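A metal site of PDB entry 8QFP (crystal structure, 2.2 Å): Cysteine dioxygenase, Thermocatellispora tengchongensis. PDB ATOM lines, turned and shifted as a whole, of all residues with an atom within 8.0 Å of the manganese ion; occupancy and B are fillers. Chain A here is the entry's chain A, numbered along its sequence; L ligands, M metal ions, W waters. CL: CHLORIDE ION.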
ATOM      1  N   ARG A  61       2.445   6.880  17.886  1.00  0.00           N
ATOM      2  CA  ARG A  61       1.420   7.026  18.913  1.00  0.00           C
ATOM      3  C   ARG A  61       1.071   5.662  19.504  1.00  0.00           C
ATOM      4  O   ARG A  61       0.847   4.695  18.781  1.00  0.00           O
ATOM      5  CB  ARG A  61       0.170   7.670  18.316  1.00  0.00           C
ATOM      6  CG  ARG A  61      -0.981   7.835  19.311  1.00  0.00           C
ATOM      7  CD  ARG A  61      -1.837   9.066  18.987  1.00  0.00           C
ATOM      8  NE  ARG A  61      -3.104   8.706  18.351  1.00  0.00           N
ATOM      9  CZ  ARG A  61      -3.397   8.970  17.080  1.00  0.00           C
ATOM     10  NH1 ARG A  61      -2.522   9.608  16.317  1.00  0.00           N
ATOM     11  NH2 ARG A  61      -4.578   8.609  16.579  1.00  0.00           N
ATOM     12  N   LEU A  77      -5.125   6.756  25.125  1.00  0.00           N
ATOM     13  CA  LEU A  77      -4.130   7.313  24.212  1.00  0.00           C
ATOM     14  C   LEU A  77      -3.074   8.067  24.996  1.00  0.00           C
ATOM     15  O   LEU A  77      -3.396   8.891  25.863  1.00  0.00           O
ATOM     16  CB  LEU A  77      -4.779   8.233  23.170  1.00  0.00           C
ATOM     17  CG  LEU A  77      -5.268   7.545  21.891  1.00  0.00           C
ATOM     18  CD1 LEU A  77      -6.235   6.413  22.210  1.00  0.00           C
ATOM     19  CD2 LEU A  77      -5.897   8.552  20.940  1.00  0.00           C
ATOM     20  N   THR A  85      -4.011  12.888  14.558  1.00  0.00           N
ATOM     21  CA  THR A  85      -5.003  11.934  14.083  1.00  0.00           C
ATOM     22  C   THR A  85      -5.345  12.130  12.609  1.00  0.00           C
ATOM     23  O   THR A  85      -5.897  11.223  11.986  1.00  0.00           O
ATOM     24  CB  THR A  85      -6.289  12.061  14.901  1.00  0.00           C
ATOM     25  OG1 THR A  85      -6.924  13.308  14.581  1.00  0.00           O
ATOM     26  CG2 THR A  85      -6.001  12.006  16.399  1.00  0.00           C
ATOM     27  N   GLY A  86      -5.035  13.289  12.045  1.00  0.00           N
ATOM     28  CA  GLY A  86      -5.575  13.659  10.745  1.00  0.00           C
ATOM     29  C   GLY A  86      -7.077  13.888  10.828  1.00  0.00           C
ATOM     30  O   GLY A  86      -7.714  13.573  11.834  1.00  0.00           O
ATOM     31  N   TRP A  87      -7.653  14.439   9.761  1.00  0.00           N
ATOM     32  CA  TRP A  87      -9.092  14.677   9.750  1.00  0.00           C
ATOM     33  C   TRP A  87      -9.844  13.364   9.586  1.00  0.00           C
ATOM     34  O   TRP A  87      -9.419  12.475   8.839  1.00  0.00           O
ATOM     35  CB  TRP A  87      -9.456  15.645   8.609  1.00  0.00           C
ATOM     36  CG  TRP A  87      -8.904  17.032   8.808  1.00  0.00           C
ATOM     37  CD1 TRP A  87      -7.812  17.566   8.192  1.00  0.00           C
ATOM     38  CD2 TRP A  87      -9.407  18.036   9.704  1.00  0.00           C
ATOM     39  NE1 TRP A  87      -7.609  18.858   8.644  1.00  0.00           N
ATOM     40  CE2 TRP A  87      -8.573  19.163   9.564  1.00  0.00           C
ATOM     41  CE3 TRP A  87     -10.480  18.091  10.587  1.00  0.00           C
ATOM     42  CZ2 TRP A  87      -8.783  20.338  10.288  1.00  0.00           C
ATOM     43  CZ3 TRP A  87     -10.685  19.259  11.307  1.00  0.00           C
ATOM     44  CH2 TRP A  87      -9.845  20.358  11.150  1.00  0.00           C
ATOM     45  N   HIS A  88     -10.961  13.229  10.306  1.00  0.00           N
ATOM     46  CA  HIS A  88     -11.678  11.957  10.304  1.00  0.00           C
ATOM     47  C   HIS A  88     -13.042  12.157  10.949  1.00  0.00           C
ATOM     48  O   HIS A  88     -13.252  13.081  11.731  1.00  0.00           O
ATOM     49  CB  HIS A  88     -10.906  10.864  11.051  1.00  0.00           C
ATOM     50  CG  HIS A  88     -10.686  11.167  12.508  1.00  0.00           C
ATOM     51  ND1 HIS A  88      -9.635  11.936  12.966  1.00  0.00           N
ATOM     52  CD2 HIS A  88     -11.382  10.785  13.614  1.00  0.00           C
ATOM     53  CE1 HIS A  88      -9.702  12.026  14.282  1.00  0.00           C
ATOM     54  NE2 HIS A  88     -10.752  11.337  14.698  1.00  0.00           N
ATOM     55  N   ASP A  89     -13.963  11.268  10.575  1.00  0.00           N
ATOM     56  CA  ASP A  89     -15.187  11.049  11.316  1.00  0.00           C
ATOM     57  C   ASP A  89     -15.179   9.636  11.872  1.00  0.00           C
ATOM     58  O   ASP A  89     -14.297   8.822  11.566  1.00  0.00           O
ATOM     59  CB  ASP A  89     -16.424  11.260  10.425  1.00  0.00           C
ATOM     60  CG  ASP A  89     -16.445  10.309   9.253  1.00  0.00           C
ATOM     61  OD1 ASP A  89     -16.595   9.084   9.491  1.00  0.00           O
ATOM     62  OD2 ASP A  89     -16.266  10.796   8.115  1.00  0.00           O
ATOM     63  N   HIS A  90     -16.180   9.338  12.682  1.00  0.00           N
ATOM     64  CA  HIS A  90     -16.319   8.031  13.313  1.00  0.00           C
ATOM     65  C   HIS A  90     -17.509   7.255  12.756  1.00  0.00           C
ATOM     66  O   HIS A  90     -18.078   6.387  13.435  1.00  0.00           O
ATOM     67  CB  HIS A  90     -16.396   8.218  14.825  1.00  0.00           C
ATOM     68  CG  HIS A  90     -15.528   9.329  15.323  1.00  0.00           C
ATOM     69  ND1 HIS A  90     -15.989  10.621  15.472  1.00  0.00           N
ATOM     70  CD2 HIS A  90     -14.205   9.363  15.616  1.00  0.00           C
ATOM     71  CE1 HIS A  90     -14.996  11.394  15.872  1.00  0.00           C
ATOM     72  NE2 HIS A  90     -13.909  10.656  15.979  1.00  0.00           N
ATOM     73  N   GLY A  95     -19.034   9.611  20.489  1.00  0.00           N
ATOM     74  CA  GLY A  95     -17.824   9.489  21.294  1.00  0.00           C
ATOM     75  C   GLY A  95     -17.678  10.585  22.325  1.00  0.00           C
ATOM     76  O   GLY A  95     -18.406  11.579  22.338  1.00  0.00           O
ATOM     77  N   VAL A  97     -14.238  12.299  24.918  1.00  0.00           N
ATOM     78  CA  VAL A  97     -12.811  12.344  25.212  1.00  0.00           C
ATOM     79  C   VAL A  97     -12.599  13.028  26.552  1.00  0.00           C
ATOM     80  O   VAL A  97     -13.187  14.092  26.812  1.00  0.00           O
ATOM     81  CB  VAL A  97     -12.031  13.078  24.107  1.00  0.00           C
ATOM     82  CG1 VAL A  97     -10.547  13.059  24.394  1.00  0.00           C
ATOM     83  CG2 VAL A  97     -12.328  12.469  22.722  1.00  0.00           C
ATOM     84  N   GLU A 106      -8.246  20.163  19.681  1.00  0.00           N
ATOM     85  CA  GLU A 106      -9.258  19.595  18.816  1.00  0.00           C
ATOM     86  C   GLU A 106      -9.593  20.615  17.742  1.00  0.00           C
ATOM     87  O   GLU A 106      -9.860  21.783  18.041  1.00  0.00           O
ATOM     88  CB  GLU A 106     -10.515  19.178  19.579  1.00  0.00           C
ATOM     89  CG  GLU A 106     -11.343  18.091  18.846  1.00  0.00           C
ATOM     90  CD  GLU A 106     -12.790  18.447  18.750  1.00  0.00           C
ATOM     91  OE1 GLU A 106     -13.158  19.539  19.225  1.00  0.00           O
ATOM     92  OE2 GLU A 106     -13.582  17.640  18.229  1.00  0.00           O
ATOM     93  N   PHE A 126     -15.019  16.294  26.490  1.00  0.00           N
ATOM     94  CA  PHE A 126     -16.043  16.702  25.535  1.00  0.00           C
ATOM     95  C   PHE A 126     -16.602  15.456  24.872  1.00  0.00           C
ATOM     96  O   PHE A 126     -16.004  14.371  24.933  1.00  0.00           O
ATOM     97  CB  PHE A 126     -15.477  17.678  24.498  1.00  0.00           C
ATOM     98  CG  PHE A 126     -14.393  17.098  23.647  1.00  0.00           C
ATOM     99  CD1 PHE A 126     -14.687  16.596  22.389  1.00  0.00           C
ATOM    100  CD2 PHE A 126     -13.077  17.091  24.065  1.00  0.00           C
ATOM    101  CE1 PHE A 126     -13.700  16.073  21.574  1.00  0.00           C
ATOM    102  CE2 PHE A 126     -12.072  16.575  23.238  1.00  0.00           C
ATOM    103  CZ  PHE A 126     -12.395  16.059  21.988  1.00  0.00           C
ATOM    104  N   PHE A 128     -19.227  14.029  21.342  1.00  0.00           N
ATOM    105  CA  PHE A 128     -19.699  14.335  20.002  1.00  0.00           C
ATOM    106  C   PHE A 128     -20.603  13.203  19.516  1.00  0.00           C
ATOM    107  O   PHE A 128     -20.497  12.055  19.958  1.00  0.00           O
ATOM    108  CB  PHE A 128     -18.534  14.517  19.019  1.00  0.00           C
ATOM    109  CG  PHE A 128     -17.508  13.421  19.097  1.00  0.00           C
ATOM    110  CD1 PHE A 128     -17.715  12.223  18.445  1.00  0.00           C
ATOM    111  CD2 PHE A 128     -16.332  13.594  19.821  1.00  0.00           C
ATOM    112  CE1 PHE A 128     -16.779  11.208  18.506  1.00  0.00           C
ATOM    113  CE2 PHE A 128     -15.385  12.585  19.887  1.00  0.00           C
ATOM    114  CZ  PHE A 128     -15.614  11.389  19.226  1.00  0.00           C
ATOM    115  N   HIS A 132     -19.765  13.926  13.551  1.00  0.00           N
ATOM    116  CA  HIS A 132     -18.631  14.769  13.906  1.00  0.00           C
ATOM    117  C   HIS A 132     -17.429  14.521  12.993  1.00  0.00           C
ATOM    118  O   HIS A 132     -17.057  13.371  12.732  1.00  0.00           O
ATOM    119  CB  HIS A 132     -18.227  14.508  15.357  1.00  0.00           C
ATOM    120  CG  HIS A 132     -17.485  15.637  16.007  1.00  0.00           C
ATOM    121  ND1 HIS A 132     -18.022  16.895  16.158  1.00  0.00           N
ATOM    122  CD2 HIS A 132     -16.260  15.689  16.579  1.00  0.00           C
ATOM    123  CE1 HIS A 132     -17.156  17.676  16.771  1.00  0.00           C
ATOM    124  NE2 HIS A 132     -16.081  16.966  17.047  1.00  0.00           N
ATOM    125  N   ILE A 133     -16.804  15.604  12.545  1.00  0.00           N
ATOM    126  CA  ILE A 133     -15.528  15.557  11.837  1.00  0.00           C
ATOM    127  C   ILE A 133     -14.534  16.375  12.645  1.00  0.00           C
ATOM    128  O   ILE A 133     -14.831  17.519  13.012  1.00  0.00           O
ATOM    129  CB  ILE A 133     -15.636  16.143  10.405  1.00  0.00           C
ATOM    130  CG1 ILE A 133     -16.709  15.426   9.586  1.00  0.00           C
ATOM    131  CG2 ILE A 133     -14.280  16.094   9.714  1.00  0.00           C
ATOM    132  CD1 ILE A 133     -16.971  16.075   8.242  1.00  0.00           C
ATOM    133  N   HIS A 134     -13.345  15.827  12.899  1.00  0.00           N
ATOM    134  CA  HIS A 134     -12.392  16.597  13.683  1.00  0.00           C
ATOM    135  C   HIS A 134     -10.990  16.042  13.517  1.00  0.00           C
ATOM    136  O   HIS A 134     -10.765  15.018  12.865  1.00  0.00           O
ATOM    137  CB  HIS A 134     -12.819  16.652  15.165  1.00  0.00           C
ATOM    138  CG  HIS A 134     -12.594  15.373  15.920  1.00  0.00           C
ATOM    139  ND1 HIS A 134     -12.584  15.316  17.294  1.00  0.00           N
ATOM    140  CD2 HIS A 134     -12.387  14.100  15.485  1.00  0.00           C
ATOM    141  CE1 HIS A 134     -12.370  14.076  17.679  1.00  0.00           C
ATOM    142  NE2 HIS A 134     -12.249  13.315  16.614  1.00  0.00           N
ATOM    143  N   ARG A 135     -10.038  16.749  14.127  1.00  0.00           N
ATOM    144  CA  ARG A 135      -8.638  16.383  14.157  1.00  0.00           C
ATOM    145  C   ARG A 135      -8.082  16.695  15.549  1.00  0.00           C
ATOM    146  O   ARG A 135      -8.276  17.802  16.062  1.00  0.00           O
ATOM    147  CB  ARG A 135      -7.863  17.143  13.093  1.00  0.00           C
ATOM    148  CG  ARG A 135      -6.454  16.655  12.852  1.00  0.00           C
ATOM    149  CD  ARG A 135      -5.841  17.429  11.720  1.00  0.00           C
ATOM    150  NE  ARG A 135      -4.597  18.062  12.118  1.00  0.00           N
ATOM    151  CZ  ARG A 135      -4.137  19.200  11.619  1.00  0.00           C
ATOM    152  NH1 ARG A 135      -4.826  19.854  10.676  1.00  0.00           N
ATOM    153  NH2 ARG A 135      -2.988  19.692  12.052  1.00  0.00           N
ATOM    154  N   LEU A 136      -7.423  15.725  16.163  1.00  0.00           N
ATOM    155  CA  LEU A 136      -6.790  15.912  17.468  1.00  0.00           C
ATOM    156  C   LEU A 136      -5.282  15.936  17.263  1.00  0.00           C
ATOM    157  O   LEU A 136      -4.719  15.025  16.637  1.00  0.00           O
ATOM    158  CB  LEU A 136      -7.191  14.807  18.443  1.00  0.00           C
ATOM    159  CG  LEU A 136      -8.634  14.838  18.961  1.00  0.00           C
ATOM    160  CD1 LEU A 136      -8.904  13.674  19.925  1.00  0.00           C
ATOM    161  CD2 LEU A 136      -8.939  16.158  19.651  1.00  0.00           C
ATOM    162  N   HIS A 147     -10.663   7.765  25.495  1.00  0.00           N
ATOM    163  CA  HIS A 147     -11.636   7.922  24.414  1.00  0.00           C
ATOM    164  C   HIS A 147     -12.604   6.753  24.449  1.00  0.00           C
ATOM    165  O   HIS A 147     -12.186   5.592  24.535  1.00  0.00           O
ATOM    166  CB  HIS A 147     -10.958   7.984  23.044  1.00  0.00           C
ATOM    167  CG  HIS A 147      -9.974   9.108  22.897  1.00  0.00           C
ATOM    168  ND1 HIS A 147      -9.994   9.979  21.825  1.00  0.00           N
ATOM    169  CD2 HIS A 147      -8.948   9.508  23.681  1.00  0.00           C
ATOM    170  CE1 HIS A 147      -9.032  10.864  21.961  1.00  0.00           C
ATOM    171  NE2 HIS A 147      -8.369  10.599  23.070  1.00  0.00           N
ATOM    172  N   TYR A 149     -16.267   5.160  22.584  1.00  0.00           N
ATOM    173  CA  TYR A 149     -17.125   5.227  21.405  1.00  0.00           C
ATOM    174  C   TYR A 149     -18.263   4.228  21.521  1.00  0.00           C
ATOM    175  O   TYR A 149     -18.075   3.104  22.005  1.00  0.00           O
ATOM    176  CB  TYR A 149     -16.340   4.957  20.111  1.00  0.00           C
ATOM    177  CG  TYR A 149     -15.101   5.828  19.940  1.00  0.00           C
ATOM    178  CD1 TYR A 149     -15.149   7.011  19.201  1.00  0.00           C
ATOM    179  CD2 TYR A 149     -13.897   5.469  20.526  1.00  0.00           C
ATOM    180  CE1 TYR A 149     -14.010   7.812  19.060  1.00  0.00           C
ATOM    181  CE2 TYR A 149     -12.764   6.250  20.387  1.00  0.00           C
ATOM    182  CZ  TYR A 149     -12.830   7.418  19.648  1.00  0.00           C
ATOM    183  OH  TYR A 149     -11.692   8.192  19.505  1.00  0.00           O
ATOM    184  N   LEU A 153     -16.137   1.701  17.534  1.00  0.00           N
ATOM    185  CA  LEU A 153     -15.394   2.329  16.435  1.00  0.00           C
ATOM    186  C   LEU A 153     -14.743   1.241  15.589  1.00  0.00           C
ATOM    187  O   LEU A 153     -13.536   0.999  15.629  1.00  0.00           O
ATOM    188  CB  LEU A 153     -14.350   3.300  16.972  1.00  0.00           C
ATOM    189  CG  LEU A 153     -13.730   4.151  15.864  1.00  0.00           C
ATOM    190  CD1 LEU A 153     -14.789   5.054  15.233  1.00  0.00           C
ATOM    191  CD2 LEU A 153     -12.550   4.972  16.356  1.00  0.00           C
ATOM    192  N   LEU A 156     -13.855   4.145  10.509  1.00  0.00           N
ATOM    193  CA  LEU A 156     -13.695   5.592  10.523  1.00  0.00           C
ATOM    194  C   LEU A 156     -13.303   6.059   9.123  1.00  0.00           C
ATOM    195  O   LEU A 156     -12.649   5.342   8.371  1.00  0.00           O
ATOM    196  CB  LEU A 156     -12.663   6.031  11.550  1.00  0.00           C
ATOM    197  CG  LEU A 156     -11.199   5.910  11.158  1.00  0.00           C
ATOM    198  CD1 LEU A 156     -10.701   7.220  10.594  1.00  0.00           C
ATOM    199  CD2 LEU A 156     -10.383   5.488  12.370  1.00  0.00           C
ATOM    200  N   GLN A 158     -11.233   8.676   6.916  1.00  0.00           N
ATOM    201  CA  GLN A 158     -10.075   9.562   6.938  1.00  0.00           C
ATOM    202  C   GLN A 158     -10.094  10.461   5.709  1.00  0.00           C
ATOM    203  O   GLN A 158     -10.088   9.968   4.570  1.00  0.00           O
ATOM    204  CB  GLN A 158      -8.782   8.751   6.993  1.00  0.00           C
ATOM    205  CG  GLN A 158      -8.484   8.170   8.388  1.00  0.00           C
ATOM    206  CD  GLN A 158      -7.998   9.217   9.385  1.00  0.00           C
ATOM    207  OE1 GLN A 158      -7.357  10.211   9.007  1.00  0.00           O
ATOM    208  NE2 GLN A 158      -8.321   9.017  10.655  1.00  0.00           N
HETATM  209 CL    CL L   1     -11.695  10.784  19.032  1.00  0.00          CL
HETATM  210 MN    MN M   1     -11.833  11.061  16.621  1.00  0.00          MN
HETATM  211  O   HOH W   1     -11.065   9.042  16.726  1.00  0.00           O
HETATM  212  O   HOH W   2      -9.857  10.860  17.236  1.00  0.00           O
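Three residues have an atom within 4 Å of the manganese ion: His 88, His 90 and His 134.
The nearest printed residue that does not touch the manganese ion is Tyr 149 (4.1 Å).
The manganese ion is bound by water W2 (2.1 Å), water W1 (2.2 Å), a ring nitrogen (NE2) of His 90 (2.2 Å), a ring nitrogen (NE2) of His 88 (2.2 Å), a ring nitrogen (NE2) of His 134 (2.3 Å) and a chlorine (CL) of the ligand (2.4 Å).
A ring nitrogen (ND1) of His 88 lies close to the side-chain hydroxyl (OG1) of Thr 85.
A ring nitrogen (ND1) of His 134 lies within hydrogen-bond range of the side-chain carboxylate (OE2) of Glu 106, 2.7 Å away.
O of Gly 86 lies within hydrogen-bond range of ND1 of His 88 (2.8 Å).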
